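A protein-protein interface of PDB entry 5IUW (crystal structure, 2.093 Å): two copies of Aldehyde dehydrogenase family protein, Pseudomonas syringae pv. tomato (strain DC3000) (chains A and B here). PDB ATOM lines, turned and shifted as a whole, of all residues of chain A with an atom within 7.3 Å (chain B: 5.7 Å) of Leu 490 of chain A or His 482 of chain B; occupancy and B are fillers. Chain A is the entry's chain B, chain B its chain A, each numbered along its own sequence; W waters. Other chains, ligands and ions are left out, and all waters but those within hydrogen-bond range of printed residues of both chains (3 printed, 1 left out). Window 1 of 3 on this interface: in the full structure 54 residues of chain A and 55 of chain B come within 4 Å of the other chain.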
ATOM      1  N   ASP A 140      11.251   1.224 -21.731  1.00  0.00           N
ATOM      2  CA  ASP A 140      12.350   0.274 -21.807  1.00  0.00           C
ATOM      3  C   ASP A 140      12.990   0.161 -20.407  1.00  0.00           C
ATOM      4  O   ASP A 140      12.346   0.490 -19.419  1.00  0.00           O
ATOM      5  CB  ASP A 140      13.341   0.698 -22.899  1.00  0.00           C
ATOM      6  CG  ASP A 140      12.778   0.465 -24.330  1.00  0.00           C
ATOM      7  OD1 ASP A 140      11.913  -0.430 -24.511  1.00  0.00           O
ATOM      8  OD2 ASP A 140      13.189   1.174 -25.275  1.00  0.00           O
ATOM      9  N   GLU A 141      14.229  -0.304 -20.308  1.00  0.00           N
ATOM     10  CA  GLU A 141      14.749  -0.723 -19.001  1.00  0.00           C
ATOM     11  C   GLU A 141      16.110  -0.145 -18.636  1.00  0.00           C
ATOM     12  O   GLU A 141      16.910   0.172 -19.501  1.00  0.00           O
ATOM     13  CB  GLU A 141      14.826  -2.254 -18.946  1.00  0.00           C
ATOM     14  CG  GLU A 141      13.461  -2.932 -19.014  1.00  0.00           C
ATOM     15  CD  GLU A 141      13.562  -4.418 -19.302  1.00  0.00           C
ATOM     16  OE1 GLU A 141      14.330  -4.789 -20.212  1.00  0.00           O
ATOM     17  OE2 GLU A 141      12.881  -5.211 -18.616  1.00  0.00           O
ATOM     18  N   VAL A 153      18.712  -0.907 -21.448  1.00  0.00           N
ATOM     19  CA  VAL A 153      18.203  -1.956 -22.303  1.00  0.00           C
ATOM     20  C   VAL A 153      17.006  -1.392 -23.045  1.00  0.00           C
ATOM     21  O   VAL A 153      15.920  -1.226 -22.464  1.00  0.00           O
ATOM     22  CB  VAL A 153      17.805  -3.218 -21.511  1.00  0.00           C
ATOM     23  CG1 VAL A 153      17.300  -4.282 -22.474  1.00  0.00           C
ATOM     24  CG2 VAL A 153      18.998  -3.733 -20.692  1.00  0.00           C
ATOM     25  N   THR A 154      17.219  -1.066 -24.316  1.00  0.00           N
ATOM     26  CA  THR A 154      16.226  -0.339 -25.089  1.00  0.00           C
ATOM     27  C   THR A 154      15.811  -1.110 -26.325  1.00  0.00           C
ATOM     28  O   THR A 154      16.468  -2.061 -26.732  1.00  0.00           O
ATOM     29  CB  THR A 154      16.746   1.037 -25.525  1.00  0.00           C
ATOM     30  OG1 THR A 154      17.913   0.860 -26.334  1.00  0.00           O
ATOM     31  CG2 THR A 154      17.089   1.891 -24.302  1.00  0.00           C
ATOM     32  N   ARG A 155      14.708  -0.671 -26.916  1.00  0.00           N
ATOM     33  CA  ARG A 155      14.181  -1.262 -28.133  1.00  0.00           C
ATOM     34  C   ARG A 155      14.232  -0.267 -29.278  1.00  0.00           C
ATOM     35  O   ARG A 155      13.992   0.928 -29.099  1.00  0.00           O
ATOM     36  CB  ARG A 155      12.753  -1.752 -27.913  1.00  0.00           C
ATOM     37  CG  ARG A 155      12.674  -2.921 -26.951  1.00  0.00           C
ATOM     38  CD  ARG A 155      11.254  -3.415 -26.772  1.00  0.00           C
ATOM     39  NE  ARG A 155      11.231  -4.743 -26.168  1.00  0.00           N
ATOM     40  CZ  ARG A 155      11.454  -5.881 -26.826  1.00  0.00           C
ATOM     41  NH1 ARG A 155      11.723  -5.882 -28.135  1.00  0.00           N
ATOM     42  NH2 ARG A 155      11.415  -7.030 -26.168  1.00  0.00           N
ATOM     43  N   GLU A 156      14.565  -0.785 -30.454  1.00  0.00           N
ATOM     44  CA  GLU A 156      14.672   0.003 -31.666  1.00  0.00           C
ATOM     45  C   GLU A 156      13.952  -0.709 -32.801  1.00  0.00           C
ATOM     46  O   GLU A 156      13.926  -1.933 -32.833  1.00  0.00           O
ATOM     47  CB  GLU A 156      16.137   0.216 -32.032  1.00  0.00           C
ATOM     48  CG  GLU A 156      16.883   1.104 -31.074  1.00  0.00           C
ATOM     49  CD  GLU A 156      18.363   1.109 -31.358  1.00  0.00           C
ATOM     50  OE1 GLU A 156      18.765   0.450 -32.335  1.00  0.00           O
ATOM     51  OE2 GLU A 156      19.109   1.776 -30.619  1.00  0.00           O
ATOM     52  N   VAL A 158      13.281  -2.507 -36.282  1.00  0.00           N
ATOM     53  CA  VAL A 158      14.174  -3.337 -37.085  1.00  0.00           C
ATOM     54  C   VAL A 158      14.539  -2.713 -38.438  1.00  0.00           C
ATOM     55  O   VAL A 158      15.626  -2.954 -38.951  1.00  0.00           O
ATOM     56  CB  VAL A 158      13.570  -4.731 -37.332  1.00  0.00           C
ATOM     57  CG1 VAL A 158      13.418  -5.469 -36.023  1.00  0.00           C
ATOM     58  CG2 VAL A 158      12.231  -4.626 -38.065  1.00  0.00           C
ATOM     59  N   ASP A 485       7.077  -6.470 -30.001  1.00  0.00           N
ATOM     60  CA  ASP A 485       8.380  -7.124 -29.939  1.00  0.00           C
ATOM     61  C   ASP A 485       8.772  -7.773 -31.265  1.00  0.00           C
ATOM     62  O   ASP A 485       9.940  -8.006 -31.522  1.00  0.00           O
ATOM     63  CB  ASP A 485       8.390  -8.174 -28.828  1.00  0.00           C
ATOM     64  CG  ASP A 485       8.174  -7.566 -27.445  1.00  0.00           C
ATOM     65  OD1 ASP A 485       8.347  -6.332 -27.283  1.00  0.00           O
ATOM     66  OD2 ASP A 485       7.834  -8.328 -26.516  1.00  0.00           O
ATOM     67  N   THR A 488      10.805  -4.929 -33.322  1.00  0.00           N
ATOM     68  CA  THR A 488      11.905  -4.231 -32.676  1.00  0.00           C
ATOM     69  C   THR A 488      13.070  -5.152 -32.281  1.00  0.00           C
ATOM     70  O   THR A 488      12.922  -6.363 -32.196  1.00  0.00           O
ATOM     71  CB  THR A 488      11.424  -3.483 -31.406  1.00  0.00           C
ATOM     72  OG1 THR A 488      10.793  -4.405 -30.526  1.00  0.00           O
ATOM     73  CG2 THR A 488      10.430  -2.390 -31.759  1.00  0.00           C
ATOM     74  N   GLU A 489      14.232  -4.543 -32.071  1.00  0.00           N
ATOM     75  CA  GLU A 489      15.435  -5.221 -31.616  1.00  0.00           C
ATOM     76  C   GLU A 489      15.854  -4.665 -30.264  1.00  0.00           C
ATOM     77  O   GLU A 489      15.829  -3.456 -30.070  1.00  0.00           O
ATOM     78  CB  GLU A 489      16.603  -5.035 -32.600  1.00  0.00           C
ATOM     79  CG  GLU A 489      16.499  -5.746 -33.934  1.00  0.00           C
ATOM     80  CD  GLU A 489      16.617  -7.257 -33.833  1.00  0.00           C
ATOM     81  OE1 GLU A 489      17.361  -7.763 -32.964  1.00  0.00           O
ATOM     82  OE2 GLU A 489      15.954  -7.945 -34.637  1.00  0.00           O
ATOM     83  N   LEU A 490      16.270  -5.542 -29.353  1.00  0.00           N
ATOM     84  CA  LEU A 490      16.839  -5.120 -28.068  1.00  0.00           C
ATOM     85  C   LEU A 490      18.302  -4.679 -28.181  1.00  0.00           C
ATOM     86  O   LEU A 490      19.090  -5.299 -28.878  1.00  0.00           O
ATOM     87  CB  LEU A 490      16.742  -6.253 -27.058  1.00  0.00           C
ATOM     88  CG  LEU A 490      15.363  -6.486 -26.465  1.00  0.00           C
ATOM     89  CD1 LEU A 490      15.297  -7.854 -25.810  1.00  0.00           C
ATOM     90  CD2 LEU A 490      15.089  -5.401 -25.440  1.00  0.00           C
ATOM     91  N   LYS A 491      18.659  -3.620 -27.465  1.00  0.00           N
ATOM     92  CA  LYS A 491      20.030  -3.154 -27.422  1.00  0.00           C
ATOM     93  C   LYS A 491      20.438  -2.923 -25.986  1.00  0.00           C
ATOM     94  O   LYS A 491      19.738  -2.239 -25.239  1.00  0.00           O
ATOM     95  CB  LYS A 491      20.216  -1.853 -28.218  1.00  0.00           C
ATOM     96  CG  LYS A 491      21.620  -1.235 -28.054  1.00  0.00           C
ATOM     97  CD  LYS A 491      21.800   0.105 -28.788  1.00  0.00           C
ATOM     98  CE  LYS A 491      21.744  -0.069 -30.305  1.00  0.00           C
ATOM     99  NZ  LYS A 491      21.776   1.247 -31.028  1.00  0.00           N
ATOM    100  N   SER A 492      21.559  -3.510 -25.601  1.00  0.00           N
ATOM    101  CA  SER A 492      22.139  -3.268 -24.292  1.00  0.00           C
ATOM    102  C   SER A 492      23.267  -2.254 -24.440  1.00  0.00           C
ATOM    103  O   SER A 492      24.300  -2.557 -25.036  1.00  0.00           O
ATOM    104  CB  SER A 492      22.669  -4.571 -23.670  1.00  0.00           C
ATOM    105  OG  SER A 492      21.629  -5.487 -23.406  1.00  0.00           O
ATOM    106  N   ALA B 450      23.747  -2.642 -33.339  1.00  0.00           N
ATOM    107  CA  ALA B 450      24.391  -3.779 -32.690  1.00  0.00           C
ATOM    108  C   ALA B 450      23.701  -4.109 -31.371  1.00  0.00           C
ATOM    109  O   ALA B 450      23.191  -3.223 -30.697  1.00  0.00           O
ATOM    110  CB  ALA B 450      25.878  -3.499 -32.470  1.00  0.00           C
ATOM    111  N   GLY B 451      23.678  -5.389 -31.012  1.00  0.00           N
ATOM    112  CA  GLY B 451      22.944  -5.835 -29.840  1.00  0.00           C
ATOM    113  C   GLY B 451      23.510  -5.329 -28.526  1.00  0.00           C
ATOM    114  O   GLY B 451      22.776  -5.133 -27.568  1.00  0.00           O
ATOM    115  N   PRO B 466      21.091  -8.263 -21.646  1.00  0.00           N
ATOM    116  CA  PRO B 466      20.765  -9.111 -22.798  1.00  0.00           C
ATOM    117  C   PRO B 466      21.879  -9.043 -23.832  1.00  0.00           C
ATOM    118  O   PRO B 466      22.425  -7.967 -24.069  1.00  0.00           O
ATOM    119  CB  PRO B 466      19.486  -8.499 -23.373  1.00  0.00           C
ATOM    120  CG  PRO B 466      19.002  -7.529 -22.385  1.00  0.00           C
ATOM    121  CD  PRO B 466      20.094  -7.205 -21.417  1.00  0.00           C
ATOM    122  N   GLY B 468      23.138 -10.481 -27.779  1.00  0.00           N
ATOM    123  CA  GLY B 468      22.725 -11.078 -29.047  1.00  0.00           C
ATOM    124  C   GLY B 468      22.755 -10.094 -30.210  1.00  0.00           C
ATOM    125  O   GLY B 468      23.088  -8.925 -30.029  1.00  0.00           O
ATOM    126  N   PHE B 470      21.942  -8.006 -33.989  1.00  0.00           N
ATOM    127  CA  PHE B 470      21.164  -7.411 -35.077  1.00  0.00           C
ATOM    128  C   PHE B 470      21.522  -8.188 -36.350  1.00  0.00           C
ATOM    129  O   PHE B 470      22.583  -8.821 -36.417  1.00  0.00           O
ATOM    130  CB  PHE B 470      21.505  -5.927 -35.285  1.00  0.00           C
ATOM    131  CG  PHE B 470      20.835  -4.964 -34.319  1.00  0.00           C
ATOM    132  CD1 PHE B 470      20.851  -5.179 -32.954  1.00  0.00           C
ATOM    133  CD2 PHE B 470      20.242  -3.797 -34.798  1.00  0.00           C
ATOM    134  CE1 PHE B 470      20.261  -4.269 -32.079  1.00  0.00           C
ATOM    135  CE2 PHE B 470      19.646  -2.884 -33.930  1.00  0.00           C
ATOM    136  CZ  PHE B 470      19.658  -3.124 -32.567  1.00  0.00           C
ATOM    137  N   ARG B 477      18.015 -13.060 -27.486  1.00  0.00           N
ATOM    138  CA  ARG B 477      19.056 -12.644 -26.572  1.00  0.00           C
ATOM    139  C   ARG B 477      19.344 -13.697 -25.514  1.00  0.00           C
ATOM    140  O   ARG B 477      18.436 -14.364 -25.024  1.00  0.00           O
ATOM    141  CB  ARG B 477      18.665 -11.321 -25.903  1.00  0.00           C
ATOM    142  CG  ARG B 477      18.370 -10.192 -26.872  1.00  0.00           C
ATOM    143  CD  ARG B 477      19.638  -9.719 -27.566  1.00  0.00           C
ATOM    144  NE  ARG B 477      19.429  -8.576 -28.461  1.00  0.00           N
ATOM    145  CZ  ARG B 477      19.340  -8.673 -29.788  1.00  0.00           C
ATOM    146  NH1 ARG B 477      19.412  -9.856 -30.385  1.00  0.00           N
ATOM    147  NH2 ARG B 477      19.186  -7.591 -30.523  1.00  0.00           N
ATOM    148  N   LYS B 479      21.362 -14.287 -21.647  1.00  0.00           N
ATOM    149  CA  LYS B 479      21.478 -13.541 -20.389  1.00  0.00           C
ATOM    150  C   LYS B 479      20.243 -12.658 -20.149  1.00  0.00           C
ATOM    151  O   LYS B 479      19.397 -12.535 -21.012  1.00  0.00           O
ATOM    152  CB  LYS B 479      22.753 -12.688 -20.355  1.00  0.00           C
ATOM    153  CG  LYS B 479      24.033 -13.482 -20.616  1.00  0.00           C
ATOM    154  CD  LYS B 479      25.269 -12.706 -20.183  1.00  0.00           C
ATOM    155  CE  LYS B 479      25.465 -11.464 -21.025  1.00  0.00           C
ATOM    156  NZ  LYS B 479      26.398 -10.512 -20.388  1.00  0.00           N
ATOM    157  N   SER B 480      20.161 -12.065 -18.955  1.00  0.00           N
ATOM    158  CA  SER B 480      19.015 -11.259 -18.497  1.00  0.00           C
ATOM    159  C   SER B 480      17.717 -12.057 -18.454  1.00  0.00           C
ATOM    160  O   SER B 480      17.704 -13.256 -18.720  1.00  0.00           O
ATOM    161  CB  SER B 480      18.832 -10.011 -19.370  1.00  0.00           C
ATOM    162  OG  SER B 480      18.058 -10.278 -20.530  1.00  0.00           O
ATOM    163  N   LEU B 481      16.631 -11.380 -18.105  1.00  0.00           N
ATOM    164  CA  LEU B 481      15.320 -12.003 -18.077  1.00  0.00           C
ATOM    165  C   LEU B 481      14.788 -12.277 -19.491  1.00  0.00           C
ATOM    166  O   LEU B 481      13.960 -13.153 -19.675  1.00  0.00           O
ATOM    167  CB  LEU B 481      14.347 -11.120 -17.292  1.00  0.00           C
ATOM    168  CG  LEU B 481      14.812 -10.808 -15.854  1.00  0.00           C
ATOM    169  CD1 LEU B 481      13.829  -9.931 -15.092  1.00  0.00           C
ATOM    170  CD2 LEU B 481      15.113 -12.085 -15.075  1.00  0.00           C
ATOM    171  N   HIS B 482      15.272 -11.527 -20.479  1.00  0.00           N
ATOM    172  CA  HIS B 482      14.804 -11.694 -21.856  1.00  0.00           C
ATOM    173  C   HIS B 482      15.173 -13.052 -22.459  1.00  0.00           C
ATOM    174  O   HIS B 482      14.529 -13.506 -23.398  1.00  0.00           O
ATOM    175  CB  HIS B 482      15.345 -10.577 -22.752  1.00  0.00           C
ATOM    176  CG  HIS B 482      14.853  -9.216 -22.372  1.00  0.00           C
ATOM    177  ND1 HIS B 482      13.640  -8.716 -22.798  1.00  0.00           N
ATOM    178  CD2 HIS B 482      15.412  -8.250 -21.603  1.00  0.00           C
ATOM    179  CE1 HIS B 482      13.476  -7.500 -22.307  1.00  0.00           C
ATOM    180  NE2 HIS B 482      14.532  -7.199 -21.572  1.00  0.00           N
ATOM    181  N   ALA B 483      16.197 -13.700 -21.917  1.00  0.00           N
ATOM    182  CA  ALA B 483      16.560 -15.035 -22.393  1.00  0.00           C
ATOM    183  C   ALA B 483      15.448 -16.052 -22.135  1.00  0.00           C
ATOM    184  O   ALA B 483      15.297 -16.997 -22.879  1.00  0.00           O
ATOM    185  CB  ALA B 483      17.841 -15.492 -21.747  1.00  0.00           C
ATOM    186  N   PHE B 484      14.671 -15.845 -21.076  1.00  0.00           N
ATOM    187  CA  PHE B 484      13.601 -16.771 -20.711  1.00  0.00           C
ATOM    188  C   PHE B 484      12.522 -16.885 -21.815  1.00  0.00           C
ATOM    189  O   PHE B 484      11.925 -17.934 -22.008  1.00  0.00           O
ATOM    190  CB  PHE B 484      12.937 -16.336 -19.393  1.00  0.00           C
ATOM    191  CG  PHE B 484      13.740 -16.652 -18.160  1.00  0.00           C
ATOM    192  CD1 PHE B 484      15.024 -16.167 -18.000  1.00  0.00           C
ATOM    193  CD2 PHE B 484      13.198 -17.417 -17.149  1.00  0.00           C
ATOM    194  CE1 PHE B 484      15.758 -16.469 -16.855  1.00  0.00           C
ATOM    195  CE2 PHE B 484      13.924 -17.716 -16.002  1.00  0.00           C
ATOM    196  CZ  PHE B 484      15.197 -17.239 -15.857  1.00  0.00           C
ATOM    197  N   ASP B 485      12.281 -15.797 -22.526  1.00  0.00           N
ATOM    198  CA  ASP B 485      11.228 -15.755 -23.528  1.00  0.00           C
ATOM    199  C   ASP B 485      11.500 -16.705 -24.697  1.00  0.00           C
ATOM    200  O   ASP B 485      10.589 -17.055 -25.439  1.00  0.00           O
ATOM    201  CB  ASP B 485      11.062 -14.324 -24.042  1.00  0.00           C
ATOM    202  CG  ASP B 485      10.608 -13.357 -22.952  1.00  0.00           C
ATOM    203  OD1 ASP B 485      10.139 -13.815 -21.878  1.00  0.00           O
ATOM    204  OD2 ASP B 485      10.734 -12.134 -23.165  1.00  0.00           O
ATOM    205  N   LYS B 486      12.748 -17.140 -24.846  1.00  0.00           N
ATOM    206  CA  LYS B 486      13.069 -18.081 -25.912  1.00  0.00           C
ATOM    207  C   LYS B 486      12.640 -19.500 -25.542  1.00  0.00           C
ATOM    208  O   LYS B 486      12.659 -20.397 -26.380  1.00  0.00           O
ATOM    209  CB  LYS B 486      14.568 -18.053 -26.215  1.00  0.00           C
ATOM    210  CG  LYS B 486      15.118 -16.671 -26.526  1.00  0.00           C
ATOM    211  CD  LYS B 486      16.553 -16.761 -27.006  1.00  0.00           C
ATOM    212  CE  LYS B 486      17.441 -17.360 -25.937  1.00  0.00           C
ATOM    213  NZ  LYS B 486      18.811 -17.545 -26.468  1.00  0.00           N
HETATM  214  O   HOH W   1      13.316  -7.786 -18.343  1.00  0.00           O
HETATM  215  O   HOH W   2      16.439 -10.095 -31.967  1.00  0.00           O
HETATM  216  O   HOH W   3      15.974  -8.361 -29.862  1.00  0.00           O
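Position printed for both chains: 485.
Of the 13 pairs that touch across the chains among the printed residues, none has its exchanged pair printed and touching as well.
Water W1 bridges the side-chain carboxylate of Glu 141 of chain A and a ring nitrogen (NE2) of His 482 of chain B.
Water W2 bridges OE1 of Glu 489 of chain A and NH1 of Arg 477 of chain B.
Water W3 lies within hydrogen-bond range of the backbone NH (N) of Leu 490 of chain A, the guanidinium group (NH2) of Arg 477 of chain B and the side-chain carboxylate (OE1) of Glu 489 of chain A.
Pro 466 of chain B touches Val 153 of chain A.
CZ of Phe 470 of chain B touches OE1 of Glu 156 of chain A, 3.7 Å away.
Glu 489 of chain A touches Phe 470 of chain B (CB to CZ, 3.6 Å).
Leu 490 of chain A touches Gly 451 of chain B (O to O, 3.9 Å).
Leu 490 of chain A touches Phe 470 of chain B.
ND1 of His 482 of chain B touches CD1 of Leu 490 of chain A (3.5 Å).
CE of Lys 491 of chain A touches O of Ala 450 of chain B, 3.5 Å away.
CA of Lys 491 of chain A touches O of Gly 451 of chain B (3.4 Å).
N of His 482 of chain B is in hydrogen-bond range of OG of Ser 480 of chain B.
O of Glu 141 of chain A lies within hydrogen-bond range of N of Val 153 of chain A (2.9 Å).
The backbone carbonyl oxygen (O) of Thr 154 of chain A is in hydrogen-bond range of the backbone NH (N) of Lys 491 of chain A (2.8 Å).
O of Glu 156 of chain A is in hydrogen-bond range of N of Glu 489 of chain A (2.7 Å).
OE2 of Glu 156 of chain A is in salt-bridge range of NZ of Lys 491 of chain A, 2.7 Å away.
Of the printed residues of chain B, Glu 141 of chain A touches His 482.
Of the printed residues of chain B, Val 153 of chain A touches Pro 466 (3.7 Å).
Of the printed residues of chain B, Glu 156 of chain A touches Phe 470.
Thr 488 of chain A touches none of the printed residues of chain B.
Of chain B, only Gly 451 (3.9 Å), Phe 470 (3.6 Å), Arg 477 (2.8 Å) and His 482 (3.5 Å) come within 4 Å of Leu 490 of chain A.
Of the printed residues of chain B, Ser 492 of chain A touches Gly 451 (2.8 Å) and Pro 466 (2.7 Å).
Of the printed residues of chain A, Phe 470 of chain B touches Glu 156, Glu 489 and Leu 490.
Leu 481 of chain B touches none of the printed residues of chain A.
His 482 of chain B touches just these residues of chain A: Glu 141 and Leu 490.
The nearest printed residue of chain B that does not touch Lys 491 of chain A is Phe 470 of chain B (4.3 Å).
Of the 13 printed residues of chain A, 7 touch a printed residue of chain B.
Of the 14 printed residues of chain B, 6 touch a printed residue of chain A.
Printed residues of chain B that touch a printed residue of chain A: Ala 450, Gly 451, Pro 466, Phe 470, Arg 477 and His 482.
Among the printed residues, 13 pairs touch across the chains.
Among the printed residues, Asp or Glu carboxylates within 4 Å of a Lys or Arg side-chain nitrogen of the other chain: Glu 489 of chain A with Arg 477 of chain B.
N of Ser 492 of chain A is in hydrogen-bond range of O of Gly 451 of chain B (2.8 Å).
The backbone carbonyl oxygen (O) of Pro 466 of chain B is in hydrogen-bond range of the side-chain hydroxyl (OG) of Ser 492 of chain A.
The side-chain carboxylate of Glu 489 of chain A lies within salt-bridge range of the guanidinium group of Arg 477 of chain B.
O of Leu 490 of chain A lies within hydrogen-bond range of NH2 of Arg 477 of chain B (2.8 Å).
A ring nitrogen (NE2) of His 482 of chain B sits at hydrogen-bond distance from the side-chain carboxylate of Glu 141 of chain A.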
